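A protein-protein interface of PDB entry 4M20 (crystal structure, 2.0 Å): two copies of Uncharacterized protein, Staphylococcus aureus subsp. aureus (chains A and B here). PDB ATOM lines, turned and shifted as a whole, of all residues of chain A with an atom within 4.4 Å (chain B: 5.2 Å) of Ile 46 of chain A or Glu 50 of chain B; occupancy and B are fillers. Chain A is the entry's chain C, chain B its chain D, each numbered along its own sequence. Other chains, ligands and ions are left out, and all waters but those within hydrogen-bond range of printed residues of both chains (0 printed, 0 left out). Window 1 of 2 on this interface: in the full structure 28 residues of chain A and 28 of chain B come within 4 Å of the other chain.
NE2 of His 41 of chain A is in hydrogen-bond range of OG1 of Thr 51 of chain B (2.9 Å). N of Gly 43 of chain A is in hydrogen-bond range of OE1 of Glu 50 of chain B. OE1 of Glu 50 of chain A sits at hydrogen-bond distance from N of Gly 43 of chain B (3.4 Å). N of Ala 75 of chain A is in hydrogen-bond range of O of Met 73 of chain B (2.8 Å). A ring nitrogen (NE2) of His 77 of chain A sits at hydrogen-bond distance from the side-chain carboxylate (OE1) of Glu 50 of chain B, 3.0 Å away.
The backbone NH (N) of Gly 43 of chain A is in hydrogen-bond range of a ring nitrogen (ND1) of His 41 of chain A (2.8 Å). The backbone carbonyl oxygen of Ala 47 of chain B is in hydrogen-bond range of the side-chain hydroxyl of Thr 51 of chain B, at 2.7 Å. The backbone carbonyl oxygen (O) of Glu 50 of chain B sits at hydrogen-bond distance from the side-chain hydroxyl (OG) of Ser 54 of chain B (2.7 Å). The backbone carbonyl oxygen of Thr 51 of chain B sits at hydrogen-bond distance from the side-chain hydroxyl of Ser 54 of chain B, at 3.1 Å.
Among the printed residues, merely in contact across the chains: His 77 of chain A with Gly 70 of chain B, Gly 42 of chain A with Glu 50 of chain B, His 41 of chain A with Ala 47 of chain B, Glu 50 of chain A with Ile 46 of chain B, Gly 43 of chain A with Ala 47 of chain B, Ala 47 of chain A with Gly 43 of chain B, Ile 46 of chain A with Glu 50 of chain B, Ile 46 of chain A with Ile 46 of chain B, Gly 43 of chain A with Gly 43 of chain B and Ile 46 of chain A with Met 73 of chain B.
Glu 50 of chain B touches just these residues of chain A: Gly 42 (3.5 Å), Gly 43 (3.5 Å), Ile 46 (3.8 Å) and His 77 (3.0 Å). Of the printed residues of chain B, Ala 75 of chain A touches Met 73. Printed residues of chain B within 4 Å of His 41 of chain A: Ala 47 (3.5 Å) and Thr 51 (2.9 Å). Printed residues of chain B within 4 Å of His 77 of chain A: Glu 50 and Gly 70. Printed residues of chain A within 4 Å of Met 73 of chain B: Ile 46 and Ala 75. Of the printed residues of chain A, Ile 46 of chain B touches Ile 46 and Glu 50. Leu 55 of chain B touches none of the printed residues of chain A. The nearest residue of chain A that does not touch Glu 50 of chain B is His 41 of chain A (4.2 Å).
Of the 14 printed residues of chain B, 7 touch a printed residue of chain A. Hydrophobic or aromatic side chains of chain B within 4 Å of the printed part of chain A: Ile 46, Ala 47 and Met 73. Printed residues of chain A that touch a printed residue of chain B: His 41, Gly 42, Gly 43, Ile 46, Ala 47, Glu 50, Ala 75 and His 77. Among the printed residues, 15 pairs touch across the chains. Among the printed residues, no Asp or Glu carboxylate lies within 4 Å of a Lys or Arg side-chain nitrogen of the other chain.
Gly 43 of chain B touches its own counterpart, Gly 43 of chain A. Gly 43 of chain A touches Ala 47 of chain B, and with the chains exchanged Ala 47 of chain A touches Gly 43 of chain B. Gly 43 of chain A touches Glu 50 of chain B, and with the chains exchanged Glu 50 of chain A touches Gly 43 of chain B. Ile 46 of chain A touches Glu 50 of chain B, and with the chains exchanged Glu 50 of chain A touches Ile 46 of chain B. Positions printed for both chains: 43, 46, 47, 48, 49, 50 and 117.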
ATOM      1  N   HIS A  41     -22.605  23.556 -11.084  1.00  0.00           N
ATOM      2  CA  HIS A  41     -23.505  22.670 -11.818  1.00  0.00           C
ATOM      3  C   HIS A  41     -24.877  22.582 -11.118  1.00  0.00           C
ATOM      4  O   HIS A  41     -24.968  22.408  -9.898  1.00  0.00           O
ATOM      5  CB  HIS A  41     -22.853  21.291 -11.946  1.00  0.00           C
ATOM      6  CG  HIS A  41     -23.473  20.395 -12.960  1.00  0.00           C
ATOM      7  ND1 HIS A  41     -24.748  19.897 -12.837  1.00  0.00           N
ATOM      8  CD2 HIS A  41     -22.945  19.828 -14.075  1.00  0.00           C
ATOM      9  CE1 HIS A  41     -24.994  19.098 -13.854  1.00  0.00           C
ATOM     10  NE2 HIS A  41     -23.923  19.045 -14.628  1.00  0.00           N
ATOM     11  N   GLY A  42     -25.944  22.726 -11.906  1.00  0.00           N
ATOM     12  CA  GLY A  42     -27.304  22.683 -11.378  1.00  0.00           C
ATOM     13  C   GLY A  42     -27.529  21.352 -10.679  1.00  0.00           C
ATOM     14  O   GLY A  42     -28.168  21.274  -9.626  1.00  0.00           O
ATOM     15  N   GLY A  43     -26.979  20.302 -11.276  1.00  0.00           N
ATOM     16  CA  GLY A  43     -27.060  18.956 -10.727  1.00  0.00           C
ATOM     17  C   GLY A  43     -26.347  18.859  -9.393  1.00  0.00           C
ATOM     18  O   GLY A  43     -26.778  18.109  -8.518  1.00  0.00           O
ATOM     19  N   ALA A  44     -25.281  19.642  -9.219  1.00  0.00           N
ATOM     20  CA  ALA A  44     -24.513  19.605  -7.979  1.00  0.00           C
ATOM     21  C   ALA A  44     -25.300  20.245  -6.840  1.00  0.00           C
ATOM     22  O   ALA A  44     -25.342  19.724  -5.718  1.00  0.00           O
ATOM     23  CB  ALA A  44     -23.187  20.299  -8.157  1.00  0.00           C
ATOM     24  N   SER A  45     -25.924  21.377  -7.145  1.00  0.00           N
ATOM     25  CA  SER A  45     -26.795  22.048  -6.200  1.00  0.00           C
ATOM     26  C   SER A  45     -27.945  21.117  -5.785  1.00  0.00           C
ATOM     27  O   SER A  45     -28.208  20.919  -4.593  1.00  0.00           O
ATOM     28  CB  SER A  45     -27.338  23.335  -6.825  1.00  0.00           C
ATOM     29  OG  SER A  45     -28.124  24.064  -5.907  1.00  0.00           O
ATOM     30  N   ILE A  46     -28.597  20.522  -6.774  1.00  0.00           N
ATOM     31  CA  ILE A  46     -29.682  19.594  -6.494  1.00  0.00           C
ATOM     32  C   ILE A  46     -29.195  18.416  -5.650  1.00  0.00           C
ATOM     33  O   ILE A  46     -29.901  17.958  -4.750  1.00  0.00           O
ATOM     34  CB  ILE A  46     -30.321  19.072  -7.784  1.00  0.00           C
ATOM     35  CG1 ILE A  46     -31.074  20.210  -8.483  1.00  0.00           C
ATOM     36  CG2 ILE A  46     -31.304  17.942  -7.481  1.00  0.00           C
ATOM     37  CD1 ILE A  46     -31.542  19.871  -9.894  1.00  0.00           C
ATOM     38  N   ALA A  47     -27.984  17.948  -5.929  1.00  0.00           N
ATOM     39  CA  ALA A  47     -27.415  16.825  -5.198  1.00  0.00           C
ATOM     40  C   ALA A  47     -27.219  17.184  -3.729  1.00  0.00           C
ATOM     41  O   ALA A  47     -27.473  16.371  -2.825  1.00  0.00           O
ATOM     42  CB  ALA A  47     -26.084  16.385  -5.843  1.00  0.00           C
ATOM     43  N   LEU A  48     -26.769  18.412  -3.497  1.00  0.00           N
ATOM     44  CA  LEU A  48     -26.665  18.943  -2.149  1.00  0.00           C
ATOM     45  C   LEU A  48     -28.017  18.959  -1.440  1.00  0.00           C
ATOM     46  O   LEU A  48     -28.125  18.580  -0.265  1.00  0.00           O
ATOM     47  CB  LEU A  48     -26.085  20.355  -2.183  1.00  0.00           C
ATOM     48  CG  LEU A  48     -25.982  21.093  -0.845  1.00  0.00           C
ATOM     49  CD1 LEU A  48     -25.001  20.405   0.075  1.00  0.00           C
ATOM     50  CD2 LEU A  48     -25.597  22.564  -1.043  1.00  0.00           C
ATOM     51  N   GLY A  49     -29.035  19.443  -2.147  1.00  0.00           N
ATOM     52  CA  GLY A  49     -30.387  19.484  -1.610  1.00  0.00           C
ATOM     53  C   GLY A  49     -30.931  18.120  -1.224  1.00  0.00           C
ATOM     54  O   GLY A  49     -31.515  17.921  -0.137  1.00  0.00           O
ATOM     55  N   GLU A  50     -30.748  17.168  -2.126  1.00  0.00           N
ATOM     56  CA  GLU A  50     -31.276  15.837  -1.918  1.00  0.00           C
ATOM     57  C   GLU A  50     -30.556  15.198  -0.730  1.00  0.00           C
ATOM     58  O   GLU A  50     -31.181  14.494   0.061  1.00  0.00           O
ATOM     59  CB  GLU A  50     -31.153  14.983  -3.180  1.00  0.00           C
ATOM     60  CG  GLU A  50     -31.614  13.560  -2.930  1.00  0.00           C
ATOM     61  CD  GLU A  50     -32.132  12.866  -4.170  1.00  0.00           C
ATOM     62  OE1 GLU A  50     -32.150  13.484  -5.259  1.00  0.00           O
ATOM     63  OE2 GLU A  50     -32.497  11.679  -4.048  1.00  0.00           O
ATOM     64  N   ALA A  75     -36.825  21.272  -8.527  1.00  0.00           N
ATOM     65  CA  ALA A  75     -35.945  22.383  -8.259  1.00  0.00           C
ATOM     66  C   ALA A  75     -36.107  23.477  -9.297  1.00  0.00           C
ATOM     67  O   ALA A  75     -36.273  23.201 -10.481  1.00  0.00           O
ATOM     68  CB  ALA A  75     -34.501  21.904  -8.235  1.00  0.00           C
ATOM     69  N   HIS A  77     -33.780  26.620 -10.498  1.00  0.00           N
ATOM     70  CA  HIS A  77     -32.480  27.295 -10.417  1.00  0.00           C
ATOM     71  C   HIS A  77     -32.701  28.794 -10.614  1.00  0.00           C
ATOM     72  O   HIS A  77     -33.262  29.201 -11.632  1.00  0.00           O
ATOM     73  CB  HIS A  77     -31.517  26.767 -11.470  1.00  0.00           C
ATOM     74  CG  HIS A  77     -31.177  25.317 -11.321  1.00  0.00           C
ATOM     75  ND1 HIS A  77     -30.786  24.759 -10.122  1.00  0.00           N
ATOM     76  CD2 HIS A  77     -31.135  24.317 -12.231  1.00  0.00           C
ATOM     77  CE1 HIS A  77     -30.524  23.476 -10.297  1.00  0.00           C
ATOM     78  NE2 HIS A  77     -30.730  23.180 -11.568  1.00  0.00           N
ATOM     79  N   MET A 117     -35.979  24.137  -3.844  1.00  0.00           N
ATOM     80  CA  MET A 117     -36.186  22.742  -4.090  1.00  0.00           C
ATOM     81  C   MET A 117     -37.307  22.202  -3.219  1.00  0.00           C
ATOM     82  O   MET A 117     -37.539  22.702  -2.105  1.00  0.00           O
ATOM     83  CB  MET A 117     -34.848  22.054  -3.825  1.00  0.00           C
ATOM     84  CG  MET A 117     -34.675  20.676  -4.303  1.00  0.00           C
ATOM     85  SD  MET A 117     -32.902  20.275  -4.320  1.00  0.00           S
ATOM     86  CE  MET A 117     -33.111  18.498  -4.380  1.00  0.00           C
ATOM     87  N   GLY B  43     -29.122  12.455  -6.442  1.00  0.00           N
ATOM     88  CA  GLY B  43     -28.559  13.690  -6.942  1.00  0.00           C
ATOM     89  C   GLY B  43     -27.568  13.496  -8.083  1.00  0.00           C
ATOM     90  O   GLY B  43     -27.464  14.360  -8.957  1.00  0.00           O
ATOM     91  N   ILE B  46     -29.638  12.763 -11.120  1.00  0.00           N
ATOM     92  CA  ILE B  46     -30.212  14.022 -11.573  1.00  0.00           C
ATOM     93  C   ILE B  46     -29.160  14.906 -12.276  1.00  0.00           C
ATOM     94  O   ILE B  46     -29.480  15.601 -13.251  1.00  0.00           O
ATOM     95  CB  ILE B  46     -30.877  14.770 -10.411  1.00  0.00           C
ATOM     96  CG1 ILE B  46     -32.133  14.001  -9.961  1.00  0.00           C
ATOM     97  CG2 ILE B  46     -31.274  16.164 -10.847  1.00  0.00           C
ATOM     98  CD1 ILE B  46     -32.779  14.528  -8.668  1.00  0.00           C
ATOM     99  N   ALA B  47     -27.924  14.899 -11.779  1.00  0.00           N
ATOM    100  CA  ALA B  47     -26.843  15.664 -12.424  1.00  0.00           C
ATOM    101  C   ALA B  47     -26.521  15.134 -13.830  1.00  0.00           C
ATOM    102  O   ALA B  47     -26.261  15.915 -14.769  1.00  0.00           O
ATOM    103  CB  ALA B  47     -25.604  15.658 -11.567  1.00  0.00           C
ATOM    104  N   LEU B  48     -26.526  13.812 -13.984  1.00  0.00           N
ATOM    105  CA  LEU B  48     -26.375  13.227 -15.319  1.00  0.00           C
ATOM    106  C   LEU B  48     -27.485  13.742 -16.227  1.00  0.00           C
ATOM    107  O   LEU B  48     -27.228  14.190 -17.341  1.00  0.00           O
ATOM    108  CB  LEU B  48     -26.380  11.694 -15.256  1.00  0.00           C
ATOM    109  CG  LEU B  48     -26.353  10.936 -16.589  1.00  0.00           C
ATOM    110  CD1 LEU B  48     -25.086  11.189 -17.358  1.00  0.00           C
ATOM    111  CD2 LEU B  48     -26.535   9.439 -16.365  1.00  0.00           C
ATOM    112  N   GLY B  49     -28.719  13.724 -15.723  1.00  0.00           N
ATOM    113  CA  GLY B  49     -29.838  14.232 -16.495  1.00  0.00           C
ATOM    114  C   GLY B  49     -29.718  15.687 -16.926  1.00  0.00           C
ATOM    115  O   GLY B  49     -30.012  16.031 -18.078  1.00  0.00           O
ATOM    116  N   GLU B  50     -29.341  16.556 -15.991  1.00  0.00           N
ATOM    117  CA  GLU B  50     -29.241  17.979 -16.291  1.00  0.00           C
ATOM    118  C   GLU B  50     -28.099  18.215 -17.292  1.00  0.00           C
ATOM    119  O   GLU B  50     -28.196  19.064 -18.194  1.00  0.00           O
ATOM    120  CB  GLU B  50     -29.060  18.804 -15.010  1.00  0.00           C
ATOM    121  CG  GLU B  50     -28.816  20.294 -15.289  1.00  0.00           C
ATOM    122  CD  GLU B  50     -29.320  21.222 -14.189  1.00  0.00           C
ATOM    123  OE1 GLU B  50     -29.874  20.736 -13.178  1.00  0.00           O
ATOM    124  OE2 GLU B  50     -29.173  22.454 -14.352  1.00  0.00           O
ATOM    125  N   THR B  51     -27.037  17.431 -17.153  1.00  0.00           N
ATOM    126  CA  THR B  51     -25.943  17.469 -18.121  1.00  0.00           C
ATOM    127  C   THR B  51     -26.471  17.140 -19.518  1.00  0.00           C
ATOM    128  O   THR B  51     -26.208  17.859 -20.482  1.00  0.00           O
ATOM    129  CB  THR B  51     -24.837  16.485 -17.737  1.00  0.00           C
ATOM    130  OG1 THR B  51     -24.379  16.790 -16.417  1.00  0.00           O
ATOM    131  CG2 THR B  51     -23.654  16.554 -18.724  1.00  0.00           C
ATOM    132  N   ALA B  52     -27.263  16.081 -19.617  1.00  0.00           N
ATOM    133  CA  ALA B  52     -27.809  15.682 -20.902  1.00  0.00           C
ATOM    134  C   ALA B  52     -28.601  16.847 -21.482  1.00  0.00           C
ATOM    135  O   ALA B  52     -28.483  17.173 -22.669  1.00  0.00           O
ATOM    136  CB  ALA B  52     -28.688  14.454 -20.749  1.00  0.00           C
ATOM    137  N   CYS B  53     -29.373  17.510 -20.625  1.00  0.00           N
ATOM    138  CA  CYS B  53     -30.218  18.602 -21.100  1.00  0.00           C
ATOM    139  C   CYS B  53     -29.480  19.786 -21.639  1.00  0.00           C
ATOM    140  O   CYS B  53     -29.786  20.293 -22.716  1.00  0.00           O
ATOM    141  CB  CYS B  53     -31.030  19.162 -19.955  1.00  0.00           C
ATOM    142  SG  CYS B  53     -32.402  18.287 -19.576  1.00  0.00           S
ATOM    143  N   SER B  54     -28.496  20.225 -20.874  1.00  0.00           N
ATOM    144  CA  SER B  54     -27.706  21.372 -21.281  1.00  0.00           C
ATOM    145  C   SER B  54     -26.894  21.081 -22.539  1.00  0.00           C
ATOM    146  O   SER B  54     -26.799  21.932 -23.417  1.00  0.00           O
ATOM    147  CB  SER B  54     -26.801  21.824 -20.137  1.00  0.00           C
ATOM    148  OG  SER B  54     -26.463  20.742 -19.295  1.00  0.00           O
ATOM    149  N   LEU B  55     -26.321  19.884 -22.636  1.00  0.00           N
ATOM    150  CA  LEU B  55     -25.591  19.531 -23.851  1.00  0.00           C
ATOM    151  C   LEU B  55     -26.496  19.551 -25.081  1.00  0.00           C
ATOM    152  O   LEU B  55     -26.132  20.105 -26.135  1.00  0.00           O
ATOM    153  CB  LEU B  55     -24.953  18.151 -23.709  1.00  0.00           C
ATOM    154  CG  LEU B  55     -23.783  17.987 -22.741  1.00  0.00           C
ATOM    155  CD1 LEU B  55     -23.352  16.525 -22.685  1.00  0.00           C
ATOM    156  CD2 LEU B  55     -22.621  18.866 -23.160  1.00  0.00           C
ATOM    157  N   GLY B  70     -29.983  25.612 -16.920  1.00  0.00           N
ATOM    158  CA  GLY B  70     -31.059  24.854 -16.312  1.00  0.00           C
ATOM    159  C   GLY B  70     -31.943  25.780 -15.510  1.00  0.00           C
ATOM    160  O   GLY B  70     -31.466  26.492 -14.633  1.00  0.00           O
ATOM    161  N   MET B  73     -35.947  21.625 -12.854  1.00  0.00           N
ATOM    162  CA  MET B  73     -35.700  20.191 -13.014  1.00  0.00           C
ATOM    163  C   MET B  73     -36.609  19.417 -12.101  1.00  0.00           C
ATOM    164  O   MET B  73     -36.767  19.784 -10.932  1.00  0.00           O
ATOM    165  CB  MET B  73     -34.254  19.817 -12.686  1.00  0.00           C
ATOM    166  CG  MET B  73     -33.203  20.483 -13.547  1.00  0.00           C
ATOM    167  SD  MET B  73     -33.113  19.716 -15.172  1.00  0.00           S
ATOM    168  CE  MET B  73     -32.550  21.140 -16.115  1.00  0.00           C
ATOM    169  N   MET B 117     -36.896  12.029 -15.576  1.00  0.00           N
ATOM    170  CA  MET B 117     -36.758  13.459 -15.362  1.00  0.00           C
ATOM    171  C   MET B 117     -37.415  14.271 -16.461  1.00  0.00           C
ATOM    172  O   MET B 117     -37.580  13.803 -17.602  1.00  0.00           O
ATOM    173  CB  MET B 117     -35.303  13.899 -15.331  1.00  0.00           C
ATOM    174  CG  MET B 117     -34.515  13.544 -14.128  1.00  0.00           C
ATOM    175  SD  MET B 117     -32.890  14.305 -14.362  1.00  0.00           S
ATOM    176  CE  MET B 117     -33.267  16.048 -14.329  1.00  0.00           C
